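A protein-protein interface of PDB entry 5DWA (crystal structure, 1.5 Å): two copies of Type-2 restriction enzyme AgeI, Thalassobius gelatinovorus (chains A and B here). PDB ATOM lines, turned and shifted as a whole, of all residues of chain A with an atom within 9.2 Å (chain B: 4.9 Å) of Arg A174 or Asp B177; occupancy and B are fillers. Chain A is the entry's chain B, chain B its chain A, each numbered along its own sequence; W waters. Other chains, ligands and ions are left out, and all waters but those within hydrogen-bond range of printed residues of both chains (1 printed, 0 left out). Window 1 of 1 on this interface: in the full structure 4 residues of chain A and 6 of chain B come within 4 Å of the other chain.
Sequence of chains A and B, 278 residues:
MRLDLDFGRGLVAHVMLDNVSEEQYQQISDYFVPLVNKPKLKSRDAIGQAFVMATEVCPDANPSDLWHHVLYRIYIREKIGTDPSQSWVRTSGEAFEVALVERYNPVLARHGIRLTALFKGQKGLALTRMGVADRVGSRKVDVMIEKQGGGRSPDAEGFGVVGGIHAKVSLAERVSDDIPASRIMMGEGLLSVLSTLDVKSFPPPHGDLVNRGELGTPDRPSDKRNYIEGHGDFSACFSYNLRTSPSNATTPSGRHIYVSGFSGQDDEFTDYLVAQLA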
ATOM      1  N   VAL A 136      -2.328  13.057 -15.552  1.00  0.00           N
ATOM      2  CA  VAL A 136      -3.551  13.785 -15.233  1.00  0.00           C
ATOM      3  C   VAL A 136      -3.481  15.194 -15.823  1.00  0.00           C
ATOM      4  O   VAL A 136      -2.482  15.898 -15.673  1.00  0.00           O
ATOM      5  CB  VAL A 136      -3.807  13.837 -13.700  1.00  0.00           C
ATOM      6  CG1 VAL A 136      -2.691  14.580 -12.967  1.00  0.00           C
ATOM      7  CG2 VAL A 136      -5.165  14.456 -13.402  1.00  0.00           C
ATOM      8  N   GLY A 137      -4.530  15.576 -16.545  1.00  0.00           N
ATOM      9  CA  GLY A 137      -4.609  16.897 -17.144  1.00  0.00           C
ATOM     10  C   GLY A 137      -3.959  17.044 -18.513  1.00  0.00           C
ATOM     11  O   GLY A 137      -4.030  18.112 -19.117  1.00  0.00           O
ATOM     12  N   LYS A 140      -5.684  18.415 -21.720  1.00  0.00           N
ATOM     13  CA  LYS A 140      -5.862  19.856 -21.865  1.00  0.00           C
ATOM     14  C   LYS A 140      -4.922  20.483 -22.904  1.00  0.00           C
ATOM     15  O   LYS A 140      -5.071  21.648 -23.260  1.00  0.00           O
ATOM     16  CB  LYS A 140      -5.664  20.542 -20.513  1.00  0.00           C
ATOM     17  CG  LYS A 140      -6.679  20.121 -19.457  1.00  0.00           C
ATOM     18  CD  LYS A 140      -8.086  20.605 -19.806  1.00  0.00           C
ATOM     19  CE  LYS A 140      -9.066  20.360 -18.658  1.00  0.00           C
ATOM     20  NZ  LYS A 140     -10.442  20.831 -18.995  1.00  0.00           N
ATOM     21  N   HIS A 166      -2.255  24.977 -24.874  1.00  0.00           N
ATOM     22  CA  HIS A 166      -3.529  24.878 -24.171  1.00  0.00           C
ATOM     23  C   HIS A 166      -4.372  26.037 -24.634  1.00  0.00           C
ATOM     24  O   HIS A 166      -4.109  27.178 -24.254  1.00  0.00           O
ATOM     25  CB  HIS A 166      -3.338  24.941 -22.651  1.00  0.00           C
ATOM     26  CG  HIS A 166      -2.404  23.905 -22.114  1.00  0.00           C
ATOM     27  ND1 HIS A 166      -2.735  23.078 -21.065  1.00  0.00           N
ATOM     28  CD2 HIS A 166      -1.148  23.565 -22.484  1.00  0.00           C
ATOM     29  CE1 HIS A 166      -1.720  22.266 -20.811  1.00  0.00           C
ATOM     30  NE2 HIS A 166      -0.750  22.536 -21.664  1.00  0.00           N
ATOM     31  N   LYS A 168      -7.828  28.031 -24.776  1.00  0.00           N
ATOM     32  CA  LYS A 168      -9.059  28.221 -24.020  1.00  0.00           C
ATOM     33  C   LYS A 168      -9.688  29.542 -24.402  1.00  0.00           C
ATOM     34  O   LYS A 168      -9.026  30.573 -24.355  1.00  0.00           O
ATOM     35  CB  LYS A 168      -8.792  28.209 -22.508  1.00  0.00           C
ATOM     36  CG  LYS A 168      -7.916  27.077 -21.996  1.00  0.00           C
ATOM     37  CD  LYS A 168      -7.708  27.211 -20.492  1.00  0.00           C
ATOM     38  CE  LYS A 168      -6.666  26.224 -19.950  1.00  0.00           C
ATOM     39  NZ  LYS A 168      -7.050  24.797 -20.144  1.00  0.00           N
ATOM     40  N   SER A 170     -12.054  31.013 -22.720  1.00  0.00           N
ATOM     41  CA  SER A 170     -12.246  31.718 -21.469  1.00  0.00           C
ATOM     42  C   SER A 170     -11.718  30.862 -20.332  1.00  0.00           C
ATOM     43  O   SER A 170     -11.485  29.669 -20.511  1.00  0.00           O
ATOM     44  CB  SER A 170     -13.724  32.062 -21.281  1.00  0.00           C
ATOM     45  OG  SER A 170     -14.532  30.924 -21.481  1.00  0.00           O
ATOM     46  N   LEU A 171     -11.539  31.468 -19.162  1.00  0.00           N
ATOM     47  CA  LEU A 171     -10.736  30.842 -18.116  1.00  0.00           C
ATOM     48  C   LEU A 171     -11.490  30.474 -16.837  1.00  0.00           C
ATOM     49  O   LEU A 171     -10.883  30.393 -15.770  1.00  0.00           O
ATOM     50  CB  LEU A 171      -9.576  31.775 -17.763  1.00  0.00           C
ATOM     51  CG  LEU A 171      -8.644  32.129 -18.925  1.00  0.00           C
ATOM     52  CD1 LEU A 171      -7.614  33.156 -18.483  1.00  0.00           C
ATOM     53  CD2 LEU A 171      -7.961  30.886 -19.472  1.00  0.00           C
ATOM     54  N   ALA A 172     -12.788  30.224 -16.922  1.00  0.00           N
ATOM     55  CA  ALA A 172     -13.545  29.879 -15.715  1.00  0.00           C
ATOM     56  C   ALA A 172     -13.171  28.481 -15.220  1.00  0.00           C
ATOM     57  O   ALA A 172     -13.386  28.147 -14.051  1.00  0.00           O
ATOM     58  CB  ALA A 172     -15.033  29.971 -15.971  1.00  0.00           C
ATOM     59  N   GLU A 173     -12.587  27.677 -16.102  1.00  0.00           N
ATOM     60  CA  GLU A 173     -12.261  26.296 -15.775  1.00  0.00           C
ATOM     61  C   GLU A 173     -11.111  26.173 -14.782  1.00  0.00           C
ATOM     62  O   GLU A 173     -10.389  27.135 -14.513  1.00  0.00           O
ATOM     63  CB  GLU A 173     -11.926  25.518 -17.046  1.00  0.00           C
ATOM     64  N   ARG A 174     -10.968  24.969 -14.241  1.00  0.00           N
ATOM     65  CA  ARG A 174      -9.924  24.628 -13.284  1.00  0.00           C
ATOM     66  C   ARG A 174      -8.564  24.506 -13.981  1.00  0.00           C
ATOM     67  O   ARG A 174      -8.138  23.408 -14.331  1.00  0.00           O
ATOM     68  CB  ARG A 174     -10.294  23.314 -12.584  1.00  0.00           C
ATOM     69  CG  ARG A 174      -9.408  22.907 -11.419  1.00  0.00           C
ATOM     70  CD  ARG A 174      -9.702  23.720 -10.176  1.00  0.00           C
ATOM     71  NE  ARG A 174     -11.105  23.674  -9.772  1.00  0.00           N
ATOM     72  CZ  ARG A 174     -11.564  24.192  -8.637  1.00  0.00           C
ATOM     73  NH1 ARG A 174     -10.726  24.780  -7.793  1.00  0.00           N
ATOM     74  NH2 ARG A 174     -12.854  24.118  -8.341  1.00  0.00           N
ATOM     75  N   VAL A 175      -7.885  25.634 -14.178  1.00  0.00           N
ATOM     76  CA  VAL A 175      -6.628  25.651 -14.930  1.00  0.00           C
ATOM     77  C   VAL A 175      -5.505  24.923 -14.168  1.00  0.00           C
ATOM     78  O   VAL A 175      -4.478  24.566 -14.746  1.00  0.00           O
ATOM     79  CB  VAL A 175      -6.208  27.110 -15.267  1.00  0.00           C
ATOM     80  CG1 VAL A 175      -4.953  27.147 -16.133  1.00  0.00           C
ATOM     81  CG2 VAL A 175      -7.341  27.825 -15.984  1.00  0.00           C
ATOM     82  N   SER A 176      -5.709  24.672 -12.880  1.00  0.00           N
ATOM     83  CA  SER A 176      -4.733  23.904 -12.112  1.00  0.00           C
ATOM     84  C   SER A 176      -4.631  22.479 -12.658  1.00  0.00           C
ATOM     85  O   SER A 176      -3.611  21.811 -12.480  1.00  0.00           O
ATOM     86  CB  SER A 176      -5.093  23.891 -10.624  1.00  0.00           C
ATOM     87  OG  SER A 176      -6.370  23.317 -10.412  1.00  0.00           O
ATOM     88  N   ASP A 177      -5.692  22.029 -13.329  1.00  0.00           N
ATOM     89  CA  ASP A 177      -5.685  20.766 -14.067  1.00  0.00           C
ATOM     90  C   ASP A 177      -4.512  20.685 -15.017  1.00  0.00           C
ATOM     91  O   ASP A 177      -3.886  19.637 -15.176  1.00  0.00           O
ATOM     92  CB  ASP A 177      -6.962  20.603 -14.889  1.00  0.00           C
ATOM     93  CG  ASP A 177      -8.154  20.233 -14.053  1.00  0.00           C
ATOM     94  OD1 ASP A 177      -8.109  20.412 -12.817  1.00  0.00           O
ATOM     95  OD2 ASP A 177      -9.137  19.755 -14.652  1.00  0.00           O
ATOM     96  N   ASP A 178      -4.238  21.811 -15.663  1.00  0.00           N
ATOM     97  CA  ASP A 178      -3.259  21.853 -16.745  1.00  0.00           C
ATOM     98  C   ASP A 178      -1.830  21.734 -16.268  1.00  0.00           C
ATOM     99  O   ASP A 178      -0.956  21.351 -17.036  1.00  0.00           O
ATOM    100  CB  ASP A 178      -3.383  23.156 -17.530  1.00  0.00           C
ATOM    101  CG  ASP A 178      -4.711  23.297 -18.218  1.00  0.00           C
ATOM    102  OD1 ASP A 178      -4.708  23.490 -19.449  1.00  0.00           O
ATOM    103  OD2 ASP A 178      -5.751  23.222 -17.530  1.00  0.00           O
ATOM    104  N   ILE A 179      -1.595  22.076 -15.007  1.00  0.00           N
ATOM    105  CA  ILE A 179      -0.242  22.344 -14.525  1.00  0.00           C
ATOM    106  C   ILE A 179       0.721  21.145 -14.549  1.00  0.00           C
ATOM    107  O   ILE A 179       1.848  21.289 -15.027  1.00  0.00           O
ATOM    108  CB  ILE A 179      -0.280  22.924 -13.089  1.00  0.00           C
ATOM    109  CG1 ILE A 179      -1.078  24.232 -13.057  1.00  0.00           C
ATOM    110  CG2 ILE A 179       1.130  23.121 -12.547  1.00  0.00           C
ATOM    111  CD1 ILE A 179      -0.882  25.121 -14.271  1.00  0.00           C
ATOM    112  N   PRO A 180       0.301  19.965 -14.042  1.00  0.00           N
ATOM    113  CA  PRO A 180       1.306  18.896 -13.963  1.00  0.00           C
ATOM    114  C   PRO A 180       1.889  18.495 -15.319  1.00  0.00           C
ATOM    115  O   PRO A 180       3.112  18.369 -15.439  1.00  0.00           O
ATOM    116  CB  PRO A 180       0.529  17.729 -13.340  1.00  0.00           C
ATOM    117  CG  PRO A 180      -0.559  18.384 -12.557  1.00  0.00           C
ATOM    118  CD  PRO A 180      -0.967  19.558 -13.407  1.00  0.00           C
ATOM    119  N   GLU A 214     -10.460  37.627 -17.169  1.00  0.00           N
ATOM    120  CA  GLU A 214     -10.396  37.019 -15.844  1.00  0.00           C
ATOM    121  C   GLU A 214      -8.983  36.939 -15.281  1.00  0.00           C
ATOM    122  O   GLU A 214      -8.748  36.219 -14.315  1.00  0.00           O
ATOM    123  CB  GLU A 214     -11.004  35.610 -15.893  1.00  0.00           C
ATOM    124  CG  GLU A 214     -12.476  35.622 -16.282  1.00  0.00           C
ATOM    125  CD  GLU A 214     -13.056  34.250 -16.599  1.00  0.00           C
ATOM    126  OE1 GLU A 214     -12.391  33.234 -16.330  1.00  0.00           O
ATOM    127  OE2 GLU A 214     -14.193  34.200 -17.128  1.00  0.00           O
ATOM    128  N   ASP A 223      -5.913  34.047  -9.520  1.00  0.00           N
ATOM    129  CA  ASP A 223      -5.194  32.797  -9.311  1.00  0.00           C
ATOM    130  C   ASP A 223      -4.601  32.296 -10.624  1.00  0.00           C
ATOM    131  O   ASP A 223      -3.521  31.710 -10.641  1.00  0.00           O
ATOM    132  CB  ASP A 223      -6.109  31.738  -8.690  1.00  0.00           C
ATOM    133  CG  ASP A 223      -6.359  31.980  -7.207  1.00  0.00           C
ATOM    134  OD1 ASP A 223      -5.488  32.588  -6.550  1.00  0.00           O
ATOM    135  OD2 ASP A 223      -7.421  31.558  -6.698  1.00  0.00           O
ATOM    136  N   LYS A 224      -5.310  32.542 -11.724  1.00  0.00           N
ATOM    137  CA  LYS A 224      -4.829  32.145 -13.042  1.00  0.00           C
ATOM    138  C   LYS A 224      -3.562  32.889 -13.428  1.00  0.00           C
ATOM    139  O   LYS A 224      -2.632  32.295 -13.963  1.00  0.00           O
ATOM    140  CB  LYS A 224      -5.905  32.374 -14.106  1.00  0.00           C
ATOM    141  CG  LYS A 224      -6.827  31.186 -14.308  1.00  0.00           C
ATOM    142  CD  LYS A 224      -8.134  31.365 -13.563  1.00  0.00           C
ATOM    143  CE  LYS A 224      -8.824  30.029 -13.351  1.00  0.00           C
ATOM    144  NZ  LYS A 224     -10.264  30.206 -13.031  1.00  0.00           N
ATOM    145  N   TYR A 227      -0.579  31.522 -11.736  1.00  0.00           N
ATOM    146  CA  TYR A 227      -0.044  30.292 -12.326  1.00  0.00           C
ATOM    147  C   TYR A 227       1.104  30.591 -13.279  1.00  0.00           C
ATOM    148  O   TYR A 227       2.111  29.886 -13.293  1.00  0.00           O
ATOM    149  CB  TYR A 227      -1.125  29.520 -13.080  1.00  0.00           C
ATOM    150  CG  TYR A 227      -2.179  28.879 -12.213  1.00  0.00           C
ATOM    151  CD1 TYR A 227      -1.890  28.455 -10.922  1.00  0.00           C
ATOM    152  CD2 TYR A 227      -3.468  28.693 -12.694  1.00  0.00           C
ATOM    153  CE1 TYR A 227      -2.864  27.865 -10.133  1.00  0.00           C
ATOM    154  CE2 TYR A 227      -4.444  28.109 -11.915  1.00  0.00           C
ATOM    155  CZ  TYR A 227      -4.137  27.695 -10.637  1.00  0.00           C
ATOM    156  OH  TYR A 227      -5.115  27.110  -9.866  1.00  0.00           O
ATOM    157  N   PHE A 234       3.531  27.728 -17.156  1.00  0.00           N
ATOM    158  CA  PHE A 234       3.510  27.652 -18.619  1.00  0.00           C
ATOM    159  C   PHE A 234       4.728  28.395 -19.139  1.00  0.00           C
ATOM    160  O   PHE A 234       5.257  29.271 -18.449  1.00  0.00           O
ATOM    161  CB  PHE A 234       2.230  28.277 -19.196  1.00  0.00           C
ATOM    162  CG  PHE A 234       0.974  27.527 -18.860  1.00  0.00           C
ATOM    163  CD1 PHE A 234       0.533  26.488 -19.668  1.00  0.00           C
ATOM    164  CD2 PHE A 234       0.217  27.876 -17.751  1.00  0.00           C
ATOM    165  CE1 PHE A 234      -0.629  25.799 -19.366  1.00  0.00           C
ATOM    166  CE2 PHE A 234      -0.954  27.189 -17.449  1.00  0.00           C
ATOM    167  CZ  PHE A 234      -1.370  26.153 -18.256  1.00  0.00           C
ATOM    168  N   ARG B 139      -8.322  22.950  -3.662  1.00  0.00           N
ATOM    169  CA  ARG B 139      -9.621  23.573  -3.392  1.00  0.00           C
ATOM    170  C   ARG B 139     -10.814  22.773  -3.908  1.00  0.00           C
ATOM    171  O   ARG B 139     -11.944  22.980  -3.457  1.00  0.00           O
ATOM    172  CB  ARG B 139      -9.678  24.979  -3.994  1.00  0.00           C
ATOM    173  CG  ARG B 139      -8.609  25.921  -3.465  1.00  0.00           C
ATOM    174  CD  ARG B 139      -9.089  27.366  -3.467  1.00  0.00           C
ATOM    175  NE  ARG B 139      -9.272  27.889  -2.115  1.00  0.00           N
ATOM    176  CZ  ARG B 139     -10.426  28.350  -1.638  1.00  0.00           C
ATOM    177  NH1 ARG B 139     -11.508  28.362  -2.403  1.00  0.00           N
ATOM    178  NH2 ARG B 139     -10.495  28.809  -0.399  1.00  0.00           N
ATOM    179  N   LYS B 140     -10.566  21.862  -4.843  1.00  0.00           N
ATOM    180  CA  LYS B 140     -11.664  21.107  -5.459  1.00  0.00           C
ATOM    181  C   LYS B 140     -12.079  19.936  -4.575  1.00  0.00           C
ATOM    182  O   LYS B 140     -11.791  18.766  -4.864  1.00  0.00           O
ATOM    183  CB  LYS B 140     -11.283  20.620  -6.866  1.00  0.00           C
ATOM    184  CG  LYS B 140     -12.417  19.964  -7.664  1.00  0.00           C
ATOM    185  CD  LYS B 140     -13.676  20.833  -7.737  1.00  0.00           C
ATOM    186  CE  LYS B 140     -14.572  20.387  -8.905  1.00  0.00           C
ATOM    187  NZ  LYS B 140     -15.945  20.951  -8.823  1.00  0.00           N
ATOM    188  N   GLU B 173     -16.138  15.348 -18.076  1.00  0.00           N
ATOM    189  CA  GLU B 173     -14.710  15.263 -17.777  1.00  0.00           C
ATOM    190  C   GLU B 173     -14.378  16.176 -16.613  1.00  0.00           C
ATOM    191  O   GLU B 173     -13.215  16.352 -16.247  1.00  0.00           O
ATOM    192  CB  GLU B 173     -13.856  15.619 -18.995  1.00  0.00           C
ATOM    193  CG  GLU B 173     -13.769  14.509 -20.034  1.00  0.00           C
ATOM    194  CD  GLU B 173     -13.248  13.197 -19.470  1.00  0.00           C
ATOM    195  OE1 GLU B 173     -12.459  13.204 -18.496  1.00  0.00           O
ATOM    196  OE2 GLU B 173     -13.639  12.145 -20.007  1.00  0.00           O
ATOM    197  N   ARG B 174     -15.418  16.743 -16.021  1.00  0.00           N
ATOM    198  CA  ARG B 174     -15.243  17.646 -14.898  1.00  0.00           C
ATOM    199  C   ARG B 174     -14.755  16.907 -13.655  1.00  0.00           C
ATOM    200  O   ARG B 174     -14.163  17.512 -12.767  1.00  0.00           O
ATOM    201  CB  ARG B 174     -16.551  18.380 -14.622  1.00  0.00           C
ATOM    202  CG  ARG B 174     -16.803  19.503 -15.610  1.00  0.00           C
ATOM    203  CD  ARG B 174     -18.158  20.135 -15.405  1.00  0.00           C
ATOM    204  NE  ARG B 174     -19.227  19.318 -15.962  1.00  0.00           N
ATOM    205  CZ  ARG B 174     -19.975  18.472 -15.266  1.00  0.00           C
ATOM    206  NH1 ARG B 174     -19.815  18.350 -13.948  1.00  0.00           N
ATOM    207  NH2 ARG B 174     -20.909  17.760 -15.883  1.00  0.00           N
ATOM    208  N   VAL B 175     -14.952  15.595 -13.608  1.00  0.00           N
ATOM    209  CA  VAL B 175     -14.476  14.828 -12.470  1.00  0.00           C
ATOM    210  C   VAL B 175     -12.939  14.818 -12.453  1.00  0.00           C
ATOM    211  O   VAL B 175     -12.318  14.630 -11.405  1.00  0.00           O
ATOM    212  CB  VAL B 175     -15.059  13.391 -12.474  1.00  0.00           C
ATOM    213  CG1 VAL B 175     -14.572  12.610 -13.689  1.00  0.00           C
ATOM    214  CG2 VAL B 175     -14.699  12.656 -11.177  1.00  0.00           C
ATOM    215  N   SER B 176     -12.326  15.038 -13.615  1.00  0.00           N
ATOM    216  CA  SER B 176     -10.874  15.148 -13.684  1.00  0.00           C
ATOM    217  C   SER B 176     -10.366  16.334 -12.861  1.00  0.00           C
ATOM    218  O   SER B 176      -9.228  16.316 -12.382  1.00  0.00           O
ATOM    219  CB  SER B 176     -10.412  15.271 -15.138  1.00  0.00           C
ATOM    220  OG  SER B 176     -10.868  14.171 -15.903  1.00  0.00           O
ATOM    221  N   ASP B 177     -11.219  17.344 -12.684  1.00  0.00           N
ATOM    222  CA  ASP B 177     -10.896  18.503 -11.841  1.00  0.00           C
ATOM    223  C   ASP B 177     -10.622  18.074 -10.405  1.00  0.00           C
ATOM    224  O   ASP B 177      -9.849  18.714  -9.692  1.00  0.00           O
ATOM    225  CB  ASP B 177     -12.032  19.542 -11.812  1.00  0.00           C
ATOM    226  CG  ASP B 177     -12.351  20.127 -13.172  1.00  0.00           C
ATOM    227  OD1 ASP B 177     -11.680  19.779 -14.165  1.00  0.00           O
ATOM    228  OD2 ASP B 177     -13.291  20.951 -13.240  1.00  0.00           O
ATOM    229  N   ASP B 178     -11.292  17.007  -9.977  1.00  0.00           N
ATOM    230  CA  ASP B 178     -11.188  16.524  -8.600  1.00  0.00           C
ATOM    231  C   ASP B 178      -9.998  15.620  -8.359  1.00  0.00           C
ATOM    232  O   ASP B 178      -9.607  15.409  -7.224  1.00  0.00           O
ATOM    233  CB  ASP B 178     -12.444  15.750  -8.209  1.00  0.00           C
ATOM    234  CG  ASP B 178     -13.680  16.615  -8.195  1.00  0.00           C
ATOM    235  OD1 ASP B 178     -14.014  17.143  -7.109  1.00  0.00           O
ATOM    236  OD2 ASP B 178     -14.306  16.759  -9.268  1.00  0.00           O
ATOM    237  N   ILE B 179      -9.425  15.061  -9.418  1.00  0.00           N
ATOM    238  CA  ILE B 179      -8.397  14.044  -9.231  1.00  0.00           C
ATOM    239  C   ILE B 179      -7.132  14.567  -8.525  1.00  0.00           C
ATOM    240  O   ILE B 179      -6.657  13.931  -7.590  1.00  0.00           O
ATOM    241  CB  ILE B 179      -8.026  13.394 -10.580  1.00  0.00           C
ATOM    242  CG1 ILE B 179      -9.193  12.540 -11.065  1.00  0.00           C
ATOM    243  CG2 ILE B 179      -6.776  12.544 -10.449  1.00  0.00           C
ATOM    244  CD1 ILE B 179      -9.021  12.029 -12.492  1.00  0.00           C
ATOM    245  N   PRO B 180      -6.602  15.736  -8.931  1.00  0.00           N
ATOM    246  CA  PRO B 180      -5.408  16.159  -8.183  1.00  0.00           C
ATOM    247  C   PRO B 180      -5.701  16.435  -6.706  1.00  0.00           C
ATOM    248  O   PRO B 180      -4.916  16.022  -5.862  1.00  0.00           O
ATOM    249  CB  PRO B 180      -4.971  17.435  -8.914  1.00  0.00           C
ATOM    250  CG  PRO B 180      -5.508  17.263 -10.309  1.00  0.00           C
ATOM    251  CD  PRO B 180      -6.836  16.593 -10.110  1.00  0.00           C
ATOM    252  N   ALA B 181      -6.816  17.092  -6.400  1.00  0.00           N
ATOM    253  CA  ALA B 181      -7.199  17.306  -5.006  1.00  0.00           C
ATOM    254  C   ALA B 181      -7.328  15.978  -4.276  1.00  0.00           C
ATOM    255  O   ALA B 181      -6.866  15.829  -3.149  1.00  0.00           O
ATOM    256  CB  ALA B 181      -8.508  18.082  -4.920  1.00  0.00           C
HETATM  257  O   HOH W   1     -13.245  25.132  -5.887  1.00  0.00           O
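The side-chain carboxylate (OD2) of Asp A177 sits close to the side-chain carboxylate (OD1) of Asp B177 (2.6 Å).
Among the printed residues, merely in contact across the chains: Arg A174 with Lys B140 (3.4 Å), Arg A174 with Asp B177 (3.8 Å), Val A136 with Ile B179 (3.9 Å) and Arg A174 with Arg B139 (3.9 Å).
Printed residues of chain B within 4 Å of Val A136: Ile B179 (3.9 Å).
Ala A172 touches none of the printed residues of chain B.
Printed residues of chain B within 4 Å of Arg A174: Arg B139, Lys B140 and Asp B177.
Ser A176 touches none of the printed residues of chain B.
Of the printed residues of chain B, Asp A177 touches Asp B177 (2.6 Å).
Of the printed residues of chain A, Arg B139 touches Arg A174 (3.9 Å).
Of the printed residues of chain A, Lys B140 touches Arg A174.
Asp B177 touches two residues of chain A.
Of the printed residues of chain A, Ile B179 touches Val A136.
The nearest printed residue of chain B that does not touch Arg A174 is Asp B178 (6.4 Å).
The nearest printed residue of chain B that does not touch Asp A177 is Ser B176 (4.1 Å).
Hydrophobic or aromatic side chains of chain B within 4 Å of the printed part of chain A: Ile B179.
Of the 21 printed residues of chain A, 3 touch a printed residue of chain B.
Printed residues of chain A that touch a printed residue of chain B: Val A136, Arg A174 and Asp A177.
Hydrophobic or aromatic side chains of chain A within 4 Å of the printed part of chain B: Val A136.
Arg A174 touches Lys B140, but with the chains exchanged Lys A140 does not touch Arg B174 (7.1 Å).
Arg A174 touches Asp B177, but with the chains exchanged Asp A177 does not touch Arg B174 (5.8 Å).
Asp A177 touches its own counterpart, Asp B177.
Positions printed for both chains: 140, 173, 174, 175, 176, 177, 178, 179 and 180.
Of the 5 pairs that touch across the chains among the printed residues, 1 has its exchanged pair printed and touching as well.
Water W1 bridges NH2 of Arg A174 (2.7 Å) and O of Arg B139 (3.5 Å).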
